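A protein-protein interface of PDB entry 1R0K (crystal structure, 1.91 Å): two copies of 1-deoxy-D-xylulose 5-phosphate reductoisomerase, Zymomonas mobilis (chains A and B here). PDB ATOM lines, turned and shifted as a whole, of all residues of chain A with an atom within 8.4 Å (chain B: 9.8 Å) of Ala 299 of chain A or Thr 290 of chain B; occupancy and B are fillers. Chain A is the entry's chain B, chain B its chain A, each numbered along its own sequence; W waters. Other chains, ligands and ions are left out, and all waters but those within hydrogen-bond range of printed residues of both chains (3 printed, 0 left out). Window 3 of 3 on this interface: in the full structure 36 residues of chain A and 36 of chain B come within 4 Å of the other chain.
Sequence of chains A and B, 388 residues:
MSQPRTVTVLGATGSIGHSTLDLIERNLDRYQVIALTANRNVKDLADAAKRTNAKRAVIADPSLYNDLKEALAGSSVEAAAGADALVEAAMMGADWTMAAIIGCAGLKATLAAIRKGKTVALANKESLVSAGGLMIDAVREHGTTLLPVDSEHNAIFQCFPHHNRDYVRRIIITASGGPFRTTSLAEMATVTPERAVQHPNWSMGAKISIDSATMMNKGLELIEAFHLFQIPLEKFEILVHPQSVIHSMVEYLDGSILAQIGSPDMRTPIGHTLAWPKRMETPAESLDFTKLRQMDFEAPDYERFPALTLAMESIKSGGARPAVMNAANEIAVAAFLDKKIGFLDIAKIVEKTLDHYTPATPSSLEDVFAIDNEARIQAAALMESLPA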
ATOM      1  N   ARG A 170     -10.451  -6.806 -12.691  1.00  0.00           N
ATOM      2  CA  ARG A 170     -11.283  -5.641 -12.964  1.00  0.00           C
ATOM      3  C   ARG A 170     -10.566  -4.340 -12.629  1.00  0.00           C
ATOM      4  O   ARG A 170      -9.680  -4.304 -11.778  1.00  0.00           O
ATOM      5  CB  ARG A 170     -12.600  -5.705 -12.174  1.00  0.00           C
ATOM      6  CG  ARG A 170     -12.435  -5.707 -10.664  1.00  0.00           C
ATOM      7  CD  ARG A 170     -13.748  -5.392  -9.915  1.00  0.00           C
ATOM      8  NE  ARG A 170     -13.592  -5.683  -8.494  1.00  0.00           N
ATOM      9  CZ  ARG A 170     -14.422  -5.301  -7.526  1.00  0.00           C
ATOM     10  NH1 ARG A 170     -15.507  -4.585  -7.791  1.00  0.00           N
ATOM     11  NH2 ARG A 170     -14.159  -5.651  -6.277  1.00  0.00           N
ATOM     12  N   ALA A 175     -15.675   7.576  -9.171  1.00  0.00           N
ATOM     13  CA  ALA A 175     -16.340   8.769  -9.673  1.00  0.00           C
ATOM     14  C   ALA A 175     -17.013   9.497  -8.525  1.00  0.00           C
ATOM     15  O   ALA A 175     -17.677   8.870  -7.705  1.00  0.00           O
ATOM     16  CB  ALA A 175     -17.393   8.381 -10.719  1.00  0.00           C
ATOM     17  N   GLY A 177     -19.427  11.405  -8.801  1.00  0.00           N
ATOM     18  CA  GLY A 177     -20.855  11.331  -9.050  1.00  0.00           C
ATOM     19  C   GLY A 177     -21.371  12.674  -9.528  1.00  0.00           C
ATOM     20  O   GLY A 177     -22.517  12.797  -9.971  1.00  0.00           O
ATOM     21  N   ARG A 181     -25.349  13.910  -8.103  1.00  0.00           N
ATOM     22  CA  ARG A 181     -25.265  12.506  -7.716  1.00  0.00           C
ATOM     23  C   ARG A 181     -26.552  11.966  -7.097  1.00  0.00           C
ATOM     24  O   ARG A 181     -26.918  10.815  -7.321  1.00  0.00           O
ATOM     25  CB  ARG A 181     -24.111  12.301  -6.724  1.00  0.00           C
ATOM     26  CG  ARG A 181     -24.023  10.886  -6.139  1.00  0.00           C
ATOM     27  CD  ARG A 181     -22.832  10.751  -5.191  1.00  0.00           C
ATOM     28  NE  ARG A 181     -22.899  11.691  -4.071  1.00  0.00           N
ATOM     29  CZ  ARG A 181     -23.516  11.456  -2.916  1.00  0.00           C
ATOM     30  NH1 ARG A 181     -24.134  10.298  -2.704  1.00  0.00           N
ATOM     31  NH2 ARG A 181     -23.504  12.378  -1.962  1.00  0.00           N
ATOM     32  N   MET A 215     -21.989  13.514 -16.116  1.00  0.00           N
ATOM     33  CA  MET A 215     -21.106  12.371 -15.962  1.00  0.00           C
ATOM     34  C   MET A 215     -20.499  11.962 -17.300  1.00  0.00           C
ATOM     35  O   MET A 215     -19.994  10.852 -17.454  1.00  0.00           O
ATOM     36  CB  MET A 215     -21.826  11.185 -15.302  1.00  0.00           C
ATOM     37  CG  MET A 215     -22.034  11.363 -13.802  1.00  0.00           C
ATOM     38  SD  MET A 215     -22.338   9.803 -12.930  1.00  0.00           S
ATOM     39  CE  MET A 215     -20.660   9.205 -12.686  1.00  0.00           C
ATOM     40  N   GLU A 237     -15.353  -1.123 -14.320  1.00  0.00           N
ATOM     41  CA  GLU A 237     -16.454  -0.816 -13.427  1.00  0.00           C
ATOM     42  C   GLU A 237     -16.327   0.629 -12.991  1.00  0.00           C
ATOM     43  O   GLU A 237     -15.223   1.120 -12.764  1.00  0.00           O
ATOM     44  CB  GLU A 237     -16.405  -1.693 -12.179  1.00  0.00           C
ATOM     45  CG  GLU A 237     -16.997  -3.074 -12.337  1.00  0.00           C
ATOM     46  CD  GLU A 237     -16.803  -3.910 -11.093  1.00  0.00           C
ATOM     47  OE1 GLU A 237     -16.730  -3.324  -9.989  1.00  0.00           O
ATOM     48  OE2 GLU A 237     -16.739  -5.152 -11.219  1.00  0.00           O
ATOM     49  N   ILE A 238     -17.455   1.314 -12.886  1.00  0.00           N
ATOM     50  CA  ILE A 238     -17.438   2.686 -12.416  1.00  0.00           C
ATOM     51  C   ILE A 238     -18.033   2.601 -11.019  1.00  0.00           C
ATOM     52  O   ILE A 238     -19.074   1.973 -10.819  1.00  0.00           O
ATOM     53  CB  ILE A 238     -18.293   3.611 -13.302  1.00  0.00           C
ATOM     54  CG1 ILE A 238     -17.690   3.670 -14.709  1.00  0.00           C
ATOM     55  CG2 ILE A 238     -18.370   5.013 -12.683  1.00  0.00           C
ATOM     56  CD1 ILE A 238     -18.521   4.477 -15.692  1.00  0.00           C
ATOM     57  N   LEU A 239     -17.349   3.192 -10.049  1.00  0.00           N
ATOM     58  CA  LEU A 239     -17.817   3.169  -8.672  1.00  0.00           C
ATOM     59  C   LEU A 239     -17.942   4.594  -8.157  1.00  0.00           C
ATOM     60  O   LEU A 239     -16.960   5.338  -8.140  1.00  0.00           O
ATOM     61  CB  LEU A 239     -16.838   2.374  -7.790  1.00  0.00           C
ATOM     62  CG  LEU A 239     -17.100   2.333  -6.276  1.00  0.00           C
ATOM     63  CD1 LEU A 239     -18.399   1.598  -5.980  1.00  0.00           C
ATOM     64  CD2 LEU A 239     -15.937   1.646  -5.568  1.00  0.00           C
ATOM     65  N   VAL A 240     -19.149   4.980  -7.751  1.00  0.00           N
ATOM     66  CA  VAL A 240     -19.360   6.323  -7.225  1.00  0.00           C
ATOM     67  C   VAL A 240     -18.786   6.375  -5.813  1.00  0.00           C
ATOM     68  O   VAL A 240     -19.091   5.537  -4.967  1.00  0.00           O
ATOM     69  CB  VAL A 240     -20.858   6.703  -7.218  1.00  0.00           C
ATOM     70  CG1 VAL A 240     -21.051   8.054  -6.543  1.00  0.00           C
ATOM     71  CG2 VAL A 240     -21.379   6.762  -8.663  1.00  0.00           C
ATOM     72  N   HIS A 241     -17.936   7.368  -5.588  1.00  0.00           N
ATOM     73  CA  HIS A 241     -17.242   7.570  -4.322  1.00  0.00           C
ATOM     74  C   HIS A 241     -17.153   9.090  -4.166  1.00  0.00           C
ATOM     75  O   HIS A 241     -16.230   9.727  -4.666  1.00  0.00           O
ATOM     76  CB  HIS A 241     -15.859   6.898  -4.439  1.00  0.00           C
ATOM     77  CG  HIS A 241     -14.886   7.283  -3.370  1.00  0.00           C
ATOM     78  ND1 HIS A 241     -15.200   7.258  -2.028  1.00  0.00           N
ATOM     79  CD2 HIS A 241     -13.597   7.686  -3.449  1.00  0.00           C
ATOM     80  CE1 HIS A 241     -14.144   7.634  -1.326  1.00  0.00           C
ATOM     81  NE2 HIS A 241     -13.158   7.899  -2.165  1.00  0.00           N
ATOM     82  N   ASP A 296     -17.379   7.045   1.384  1.00  0.00           N
ATOM     83  CA  ASP A 296     -18.639   6.460   0.938  1.00  0.00           C
ATOM     84  C   ASP A 296     -18.529   5.861  -0.458  1.00  0.00           C
ATOM     85  O   ASP A 296     -17.772   6.352  -1.292  1.00  0.00           O
ATOM     86  CB  ASP A 296     -19.740   7.519   0.931  1.00  0.00           C
ATOM     87  CG  ASP A 296     -20.050   8.032   2.310  1.00  0.00           C
ATOM     88  OD1 ASP A 296     -20.486   7.214   3.147  1.00  0.00           O
ATOM     89  OD2 ASP A 296     -19.852   9.244   2.553  1.00  0.00           O
ATOM     90  N   PHE A 297     -19.299   4.806  -0.706  1.00  0.00           N
ATOM     91  CA  PHE A 297     -19.303   4.146  -2.008  1.00  0.00           C
ATOM     92  C   PHE A 297     -20.720   3.710  -2.374  1.00  0.00           C
ATOM     93  O   PHE A 297     -21.479   3.268  -1.517  1.00  0.00           O
ATOM     94  CB  PHE A 297     -18.387   2.913  -2.002  1.00  0.00           C
ATOM     95  CG  PHE A 297     -16.994   3.196  -1.536  1.00  0.00           C
ATOM     96  CD1 PHE A 297     -16.675   3.119  -0.183  1.00  0.00           C
ATOM     97  CD2 PHE A 297     -16.004   3.562  -2.444  1.00  0.00           C
ATOM     98  CE1 PHE A 297     -15.385   3.404   0.260  1.00  0.00           C
ATOM     99  CE2 PHE A 297     -14.714   3.851  -2.015  1.00  0.00           C
ATOM    100  CZ  PHE A 297     -14.402   3.771  -0.659  1.00  0.00           C
ATOM    101  N   GLU A 298     -21.069   3.839  -3.649  1.00  0.00           N
ATOM    102  CA  GLU A 298     -22.392   3.448  -4.123  1.00  0.00           C
ATOM    103  C   GLU A 298     -22.312   3.121  -5.609  1.00  0.00           C
ATOM    104  O   GLU A 298     -21.370   3.521  -6.295  1.00  0.00           O
ATOM    105  CB  GLU A 298     -23.404   4.578  -3.883  1.00  0.00           C
ATOM    106  CG  GLU A 298     -23.160   5.823  -4.722  1.00  0.00           C
ATOM    107  CD  GLU A 298     -24.138   6.943  -4.415  1.00  0.00           C
ATOM    108  OE1 GLU A 298     -24.030   7.560  -3.336  1.00  0.00           O
ATOM    109  OE2 GLU A 298     -25.023   7.209  -5.252  1.00  0.00           O
ATOM    110  N   ALA A 299     -23.302   2.392  -6.108  1.00  0.00           N
ATOM    111  CA  ALA A 299     -23.315   2.015  -7.513  1.00  0.00           C
ATOM    112  C   ALA A 299     -23.689   3.193  -8.398  1.00  0.00           C
ATOM    113  O   ALA A 299     -24.450   4.071  -7.999  1.00  0.00           O
ATOM    114  CB  ALA A 299     -24.300   0.866  -7.740  1.00  0.00           C
ATOM    115  N   PRO A 300     -23.133   3.241  -9.610  1.00  0.00           N
ATOM    116  CA  PRO A 300     -23.483   4.355 -10.487  1.00  0.00           C
ATOM    117  C   PRO A 300     -24.912   4.100 -10.973  1.00  0.00           C
ATOM    118  O   PRO A 300     -25.388   2.962 -10.944  1.00  0.00           O
ATOM    119  CB  PRO A 300     -22.448   4.242 -11.600  1.00  0.00           C
ATOM    120  CG  PRO A 300     -22.233   2.760 -11.697  1.00  0.00           C
ATOM    121  CD  PRO A 300     -22.139   2.353 -10.244  1.00  0.00           C
ATOM    122  N   ASP A 301     -25.603   5.145 -11.402  1.00  0.00           N
ATOM    123  CA  ASP A 301     -26.968   4.982 -11.883  1.00  0.00           C
ATOM    124  C   ASP A 301     -26.991   5.232 -13.385  1.00  0.00           C
ATOM    125  O   ASP A 301     -27.031   6.376 -13.829  1.00  0.00           O
ATOM    126  CB  ASP A 301     -27.899   5.970 -11.178  1.00  0.00           C
ATOM    127  CG  ASP A 301     -29.363   5.689 -11.459  1.00  0.00           C
ATOM    128  OD1 ASP A 301     -29.683   5.272 -12.589  1.00  0.00           O
ATOM    129  OD2 ASP A 301     -30.193   5.896 -10.554  1.00  0.00           O
ATOM    130  N   TYR A 302     -26.962   4.156 -14.165  1.00  0.00           N
ATOM    131  CA  TYR A 302     -26.964   4.270 -15.619  1.00  0.00           C
ATOM    132  C   TYR A 302     -28.263   4.854 -16.170  1.00  0.00           C
ATOM    133  O   TYR A 302     -28.286   5.408 -17.271  1.00  0.00           O
ATOM    134  CB  TYR A 302     -26.672   2.903 -16.242  1.00  0.00           C
ATOM    135  CG  TYR A 302     -25.217   2.507 -16.096  1.00  0.00           C
ATOM    136  CD1 TYR A 302     -24.267   2.923 -17.028  1.00  0.00           C
ATOM    137  CD2 TYR A 302     -24.777   1.773 -14.992  1.00  0.00           C
ATOM    138  CE1 TYR A 302     -22.911   2.620 -16.867  1.00  0.00           C
ATOM    139  CE2 TYR A 302     -23.420   1.466 -14.818  1.00  0.00           C
ATOM    140  CZ  TYR A 302     -22.496   1.895 -15.761  1.00  0.00           C
ATOM    141  OH  TYR A 302     -21.158   1.602 -15.606  1.00  0.00           O
ATOM    142  N   ARG A 304     -30.122   7.328 -14.613  1.00  0.00           N
ATOM    143  CA  ARG A 304     -30.081   8.771 -14.416  1.00  0.00           C
ATOM    144  C   ARG A 304     -28.945   9.468 -15.166  1.00  0.00           C
ATOM    145  O   ARG A 304     -29.010  10.669 -15.422  1.00  0.00           O
ATOM    146  CB  ARG A 304     -30.018   9.074 -12.919  1.00  0.00           C
ATOM    147  CG  ARG A 304     -31.352   8.818 -12.213  1.00  0.00           C
ATOM    148  CD  ARG A 304     -31.212   8.735 -10.701  1.00  0.00           C
ATOM    149  NE  ARG A 304     -30.539   9.900 -10.150  1.00  0.00           N
ATOM    150  CZ  ARG A 304     -29.396   9.851  -9.477  1.00  0.00           C
ATOM    151  NH1 ARG A 304     -28.790   8.690  -9.269  1.00  0.00           N
ATOM    152  NH2 ARG A 304     -28.857  10.970  -9.012  1.00  0.00           N
ATOM    153  N   PHE A 305     -27.912   8.715 -15.530  1.00  0.00           N
ATOM    154  CA  PHE A 305     -26.790   9.293 -16.259  1.00  0.00           C
ATOM    155  C   PHE A 305     -26.498   8.478 -17.520  1.00  0.00           C
ATOM    156  O   PHE A 305     -25.495   7.773 -17.605  1.00  0.00           O
ATOM    157  CB  PHE A 305     -25.562   9.374 -15.339  1.00  0.00           C
ATOM    158  CG  PHE A 305     -25.813  10.167 -14.085  1.00  0.00           C
ATOM    159  CD1 PHE A 305     -26.235   9.536 -12.917  1.00  0.00           C
ATOM    160  CD2 PHE A 305     -25.700  11.554 -14.095  1.00  0.00           C
ATOM    161  CE1 PHE A 305     -26.547  10.279 -11.772  1.00  0.00           C
ATOM    162  CE2 PHE A 305     -26.010  12.310 -12.954  1.00  0.00           C
ATOM    163  CZ  PHE A 305     -26.435  11.668 -11.790  1.00  0.00           C
ATOM    164  N   LEU A 308     -23.154   7.582 -19.471  1.00  0.00           N
ATOM    165  CA  LEU A 308     -22.298   6.447 -19.146  1.00  0.00           C
ATOM    166  C   LEU A 308     -22.562   5.313 -20.126  1.00  0.00           C
ATOM    167  O   LEU A 308     -21.632   4.650 -20.586  1.00  0.00           O
ATOM    168  CB  LEU A 308     -22.537   5.975 -17.702  1.00  0.00           C
ATOM    169  CG  LEU A 308     -22.131   6.963 -16.599  1.00  0.00           C
ATOM    170  CD1 LEU A 308     -22.380   6.334 -15.228  1.00  0.00           C
ATOM    171  CD2 LEU A 308     -20.656   7.341 -16.755  1.00  0.00           C
ATOM    172  N   SER B 286     -14.279 -11.131  -4.418  1.00  0.00           N
ATOM    173  CA  SER B 286     -13.935  -9.776  -4.837  1.00  0.00           C
ATOM    174  C   SER B 286     -14.749  -8.833  -3.959  1.00  0.00           C
ATOM    175  O   SER B 286     -15.974  -8.947  -3.891  1.00  0.00           O
ATOM    176  CB  SER B 286     -14.287  -9.547  -6.309  1.00  0.00           C
ATOM    177  OG  SER B 286     -13.470 -10.334  -7.154  1.00  0.00           O
ATOM    178  N   LEU B 287     -14.072  -7.912  -3.281  1.00  0.00           N
ATOM    179  CA  LEU B 287     -14.754  -6.977  -2.395  1.00  0.00           C
ATOM    180  C   LEU B 287     -15.818  -6.172  -3.122  1.00  0.00           C
ATOM    181  O   LEU B 287     -15.548  -5.555  -4.149  1.00  0.00           O
ATOM    182  CB  LEU B 287     -13.748  -6.021  -1.749  1.00  0.00           C
ATOM    183  CG  LEU B 287     -14.349  -5.059  -0.722  1.00  0.00           C
ATOM    184  CD1 LEU B 287     -14.923  -5.858   0.430  1.00  0.00           C
ATOM    185  CD2 LEU B 287     -13.286  -4.087  -0.227  1.00  0.00           C
ATOM    186  N   ASP B 288     -17.035  -6.198  -2.590  1.00  0.00           N
ATOM    187  CA  ASP B 288     -18.151  -5.461  -3.179  1.00  0.00           C
ATOM    188  C   ASP B 288     -18.259  -4.128  -2.444  1.00  0.00           C
ATOM    189  O   ASP B 288     -18.817  -4.060  -1.351  1.00  0.00           O
ATOM    190  CB  ASP B 288     -19.452  -6.247  -3.008  1.00  0.00           C
ATOM    191  CG  ASP B 288     -20.611  -5.622  -3.761  1.00  0.00           C
ATOM    192  OD1 ASP B 288     -20.755  -4.383  -3.711  1.00  0.00           O
ATOM    193  OD2 ASP B 288     -21.379  -6.370  -4.399  1.00  0.00           O
ATOM    194  N   PHE B 289     -17.721  -3.071  -3.042  1.00  0.00           N
ATOM    195  CA  PHE B 289     -17.747  -1.759  -2.411  1.00  0.00           C
ATOM    196  C   PHE B 289     -19.149  -1.202  -2.227  1.00  0.00           C
ATOM    197  O   PHE B 289     -19.404  -0.478  -1.261  1.00  0.00           O
ATOM    198  CB  PHE B 289     -16.904  -0.760  -3.208  1.00  0.00           C
ATOM    199  CG  PHE B 289     -15.437  -1.067  -3.201  1.00  0.00           C
ATOM    200  CD1 PHE B 289     -14.896  -1.975  -4.106  1.00  0.00           C
ATOM    201  CD2 PHE B 289     -14.591  -0.451  -2.281  1.00  0.00           C
ATOM    202  CE1 PHE B 289     -13.530  -2.267  -4.093  1.00  0.00           C
ATOM    203  CE2 PHE B 289     -13.223  -0.737  -2.260  1.00  0.00           C
ATOM    204  CZ  PHE B 289     -12.693  -1.644  -3.165  1.00  0.00           C
ATOM    205  N   THR B 290     -20.058  -1.530  -3.140  1.00  0.00           N
ATOM    206  CA  THR B 290     -21.424  -1.033  -3.023  1.00  0.00           C
ATOM    207  C   THR B 290     -22.091  -1.628  -1.788  1.00  0.00           C
ATOM    208  O   THR B 290     -22.832  -0.941  -1.083  1.00  0.00           O
ATOM    209  CB  THR B 290     -22.266  -1.355  -4.281  1.00  0.00           C
ATOM    210  OG1 THR B 290     -22.367  -2.772  -4.451  1.00  0.00           O
ATOM    211  CG2 THR B 290     -21.629  -0.741  -5.524  1.00  0.00           C
ATOM    212  N   LYS B 291     -21.824  -2.901  -1.512  1.00  0.00           N
ATOM    213  CA  LYS B 291     -22.409  -3.530  -0.332  1.00  0.00           C
ATOM    214  C   LYS B 291     -21.689  -3.049   0.926  1.00  0.00           C
ATOM    215  O   LYS B 291     -22.302  -2.911   1.985  1.00  0.00           O
ATOM    216  CB  LYS B 291     -22.356  -5.053  -0.453  1.00  0.00           C
ATOM    217  CG  LYS B 291     -23.215  -5.566  -1.602  1.00  0.00           C
ATOM    218  CD  LYS B 291     -23.411  -7.071  -1.552  1.00  0.00           C
ATOM    219  CE  LYS B 291     -24.371  -7.528  -2.646  1.00  0.00           C
ATOM    220  NZ  LYS B 291     -24.655  -8.988  -2.563  1.00  0.00           N
ATOM    221  N   LEU B 292     -20.391  -2.782   0.807  1.00  0.00           N
ATOM    222  CA  LEU B 292     -19.610  -2.283   1.937  1.00  0.00           C
ATOM    223  C   LEU B 292     -20.203  -0.934   2.328  1.00  0.00           C
ATOM    224  O   LEU B 292     -20.410  -0.643   3.506  1.00  0.00           O
ATOM    225  CB  LEU B 292     -18.150  -2.098   1.530  1.00  0.00           C
ATOM    226  CG  LEU B 292     -17.234  -1.389   2.532  1.00  0.00           C
ATOM    227  CD1 LEU B 292     -17.134  -2.192   3.825  1.00  0.00           C
ATOM    228  CD2 LEU B 292     -15.858  -1.207   1.894  1.00  0.00           C
ATOM    229  N   ARG B 293     -20.463  -0.118   1.312  1.00  0.00           N
ATOM    230  CA  ARG B 293     -21.064   1.199   1.479  1.00  0.00           C
ATOM    231  C   ARG B 293     -20.190   2.268   2.128  1.00  0.00           C
ATOM    232  O   ARG B 293     -20.104   3.384   1.612  1.00  0.00           O
ATOM    233  CB  ARG B 293     -22.389   1.064   2.244  1.00  0.00           C
ATOM    234  CG  ARG B 293     -23.107   2.378   2.475  1.00  0.00           C
ATOM    235  CD  ARG B 293     -24.490   2.161   3.083  1.00  0.00           C
ATOM    236  NE  ARG B 293     -25.071   3.415   3.556  1.00  0.00           N
ATOM    237  CZ  ARG B 293     -24.596   4.116   4.582  1.00  0.00           C
ATOM    238  NH1 ARG B 293     -25.182   5.250   4.946  1.00  0.00           N
ATOM    239  NH2 ARG B 293     -23.538   3.678   5.252  1.00  0.00           N
ATOM    240  N   GLN B 294     -19.545   1.943   3.249  1.00  0.00           N
ATOM    241  CA  GLN B 294     -18.699   2.917   3.945  1.00  0.00           C
ATOM    242  C   GLN B 294     -17.418   2.358   4.554  1.00  0.00           C
ATOM    243  O   GLN B 294     -17.327   1.175   4.884  1.00  0.00           O
ATOM    244  CB  GLN B 294     -19.463   3.593   5.090  1.00  0.00           C
ATOM    245  CG  GLN B 294     -20.624   4.469   4.709  1.00  0.00           C
ATOM    246  CD  GLN B 294     -21.186   5.199   5.920  1.00  0.00           C
ATOM    247  OE1 GLN B 294     -21.479   4.578   6.947  1.00  0.00           O
ATOM    248  NE2 GLN B 294     -21.332   6.517   5.811  1.00  0.00           N
ATOM    249  N   MET B 295     -16.445   3.250   4.717  1.00  0.00           N
ATOM    250  CA  MET B 295     -15.156   2.941   5.333  1.00  0.00           C
ATOM    251  C   MET B 295     -14.913   4.041   6.358  1.00  0.00           C
ATOM    252  O   MET B 295     -15.041   5.223   6.037  1.00  0.00           O
ATOM    253  CB  MET B 295     -14.016   2.986   4.317  1.00  0.00           C
ATOM    254  CG  MET B 295     -13.868   1.765   3.437  1.00  0.00           C
ATOM    255  SD  MET B 295     -12.449   1.981   2.339  1.00  0.00           S
ATOM    256  CE  MET B 295     -12.751   0.683   1.118  1.00  0.00           C
HETATM  257  O   HOH W   1     -14.235  -8.708  -9.268  1.00  0.00           O
HETATM  258  O   HOH W   2     -17.659  -3.229  -6.101  1.00  0.00           O
HETATM  259  O   HOH W   3     -23.815   1.898  -1.396  1.00  0.00           O
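Water W3 lies within hydrogen-bond range of O of Phe 297 of chain A (2.7 Å) and O of Thr 290 of chain B (3.0 Å).
Water W1 lies within hydrogen-bond range of OG of Ser 286 of chain B (2.8 Å) and NE of Arg 170 of chain A (3.2 Å).
Water W2 bridges the guanidinium group of Arg 170 of chain A (3.1 Å) and the backbone NH of Phe 289 of chain B (3.1 Å).
OD1 of Asp 288 of chain B is in hydrogen-bond range of N of Thr 290 of chain B, 3.0 Å away.
NH1 of Arg 170 of chain A is in salt-bridge range of OE1 of Glu 237 of chain A.
The backbone NH (N) of Ala 175 of chain A sits at hydrogen-bond distance from the backbone carbonyl oxygen (O) of Leu 239 of chain A, 2.8 Å away.
OE1 of Glu 298 of chain A lies within salt-bridge range of NH1 of Arg 181 of chain A, at 2.8 Å.
O of Val 240 of chain A sits at hydrogen-bond distance from N of Glu 298 of chain A.
A ring nitrogen (ND1) of His 241 of chain A lies within hydrogen-bond range of the backbone carbonyl oxygen of Asp 296 of chain A (2.8 Å).
Of the 10 printed residues of chain B, 7 touch a printed residue of chain A.
Hydrophobic or aromatic side chains of chain B that line the printed part of chain A: Phe 289 and Met 295.
Printed residues of chain A that touch a printed residue of chain B: Arg 170, Leu 239, Asp 296, Phe 297, Glu 298 and Ala 299.
Among the printed residues, 10 pairs touch across the chains.
Among the printed residues, no Asp or Glu carboxylate lies within 4 Å of a Lys or Arg side-chain nitrogen of the other chain.
Printed residues of chain B within 4 Å of Leu 239 of chain A: Phe 289.
Printed residues of chain B within 4 Å of Asp 296 of chain A: Arg 293 and Gln 294.
Ala 299 of chain A touches just one residue of chain B: Thr 290 (3.6 Å).
No residue of chain B comes within 4 Å of Pro 300 of chain A.
Arg 304 of chain A touches none of the printed residues of chain B.
Of the printed residues of chain A, Ser 286 of chain B touches Arg 170 (3.9 Å).
Lys 291 of chain B touches none of the printed residues of chain A.
Of the printed residues of chain A, Met 295 of chain B touches Phe 297 (3.9 Å).
The nearest printed residue of chain A that does not touch Thr 290 of chain B is Leu 239 of chain A (4.01 Å).
The nearest printed residue of chain B that does not touch Glu 298 of chain A is Phe 289 of chain B (5.2 Å).
No position is printed for both chains.
The guanidinium group (NH2) of Arg 170 of chain A lies within hydrogen-bond range of the backbone carbonyl oxygen (O) of Leu 287 of chain B, at 2.5 Å.
N of Phe 297 of chain A sits at hydrogen-bond distance from O of Arg 293 of chain B (2.8 Å).
NE2 of Gln 294 of chain B sits at hydrogen-bond distance from OD1 of Asp 296 of chain A (2.9 Å).
Ser 286 of chain B touches Arg 170 of chain A (CB to NH2, 3.9 Å).
Leu 239 of chain A touches Phe 289 of chain B.
CA of Asp 296 of chain A touches O of Arg 293 of chain B, at 3.5 Å.
CB of Phe 297 of chain A touches O of Phe 289 of chain B, at 3.6 Å.
Phe 297 of chain A touches Met 295 of chain B (CE1 to SD, 3.9 Å).
Glu 298 of chain A touches Thr 290 of chain B.
CG2 of Thr 290 of chain B touches N of Ala 299 of chain A, 3.6 Å away.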
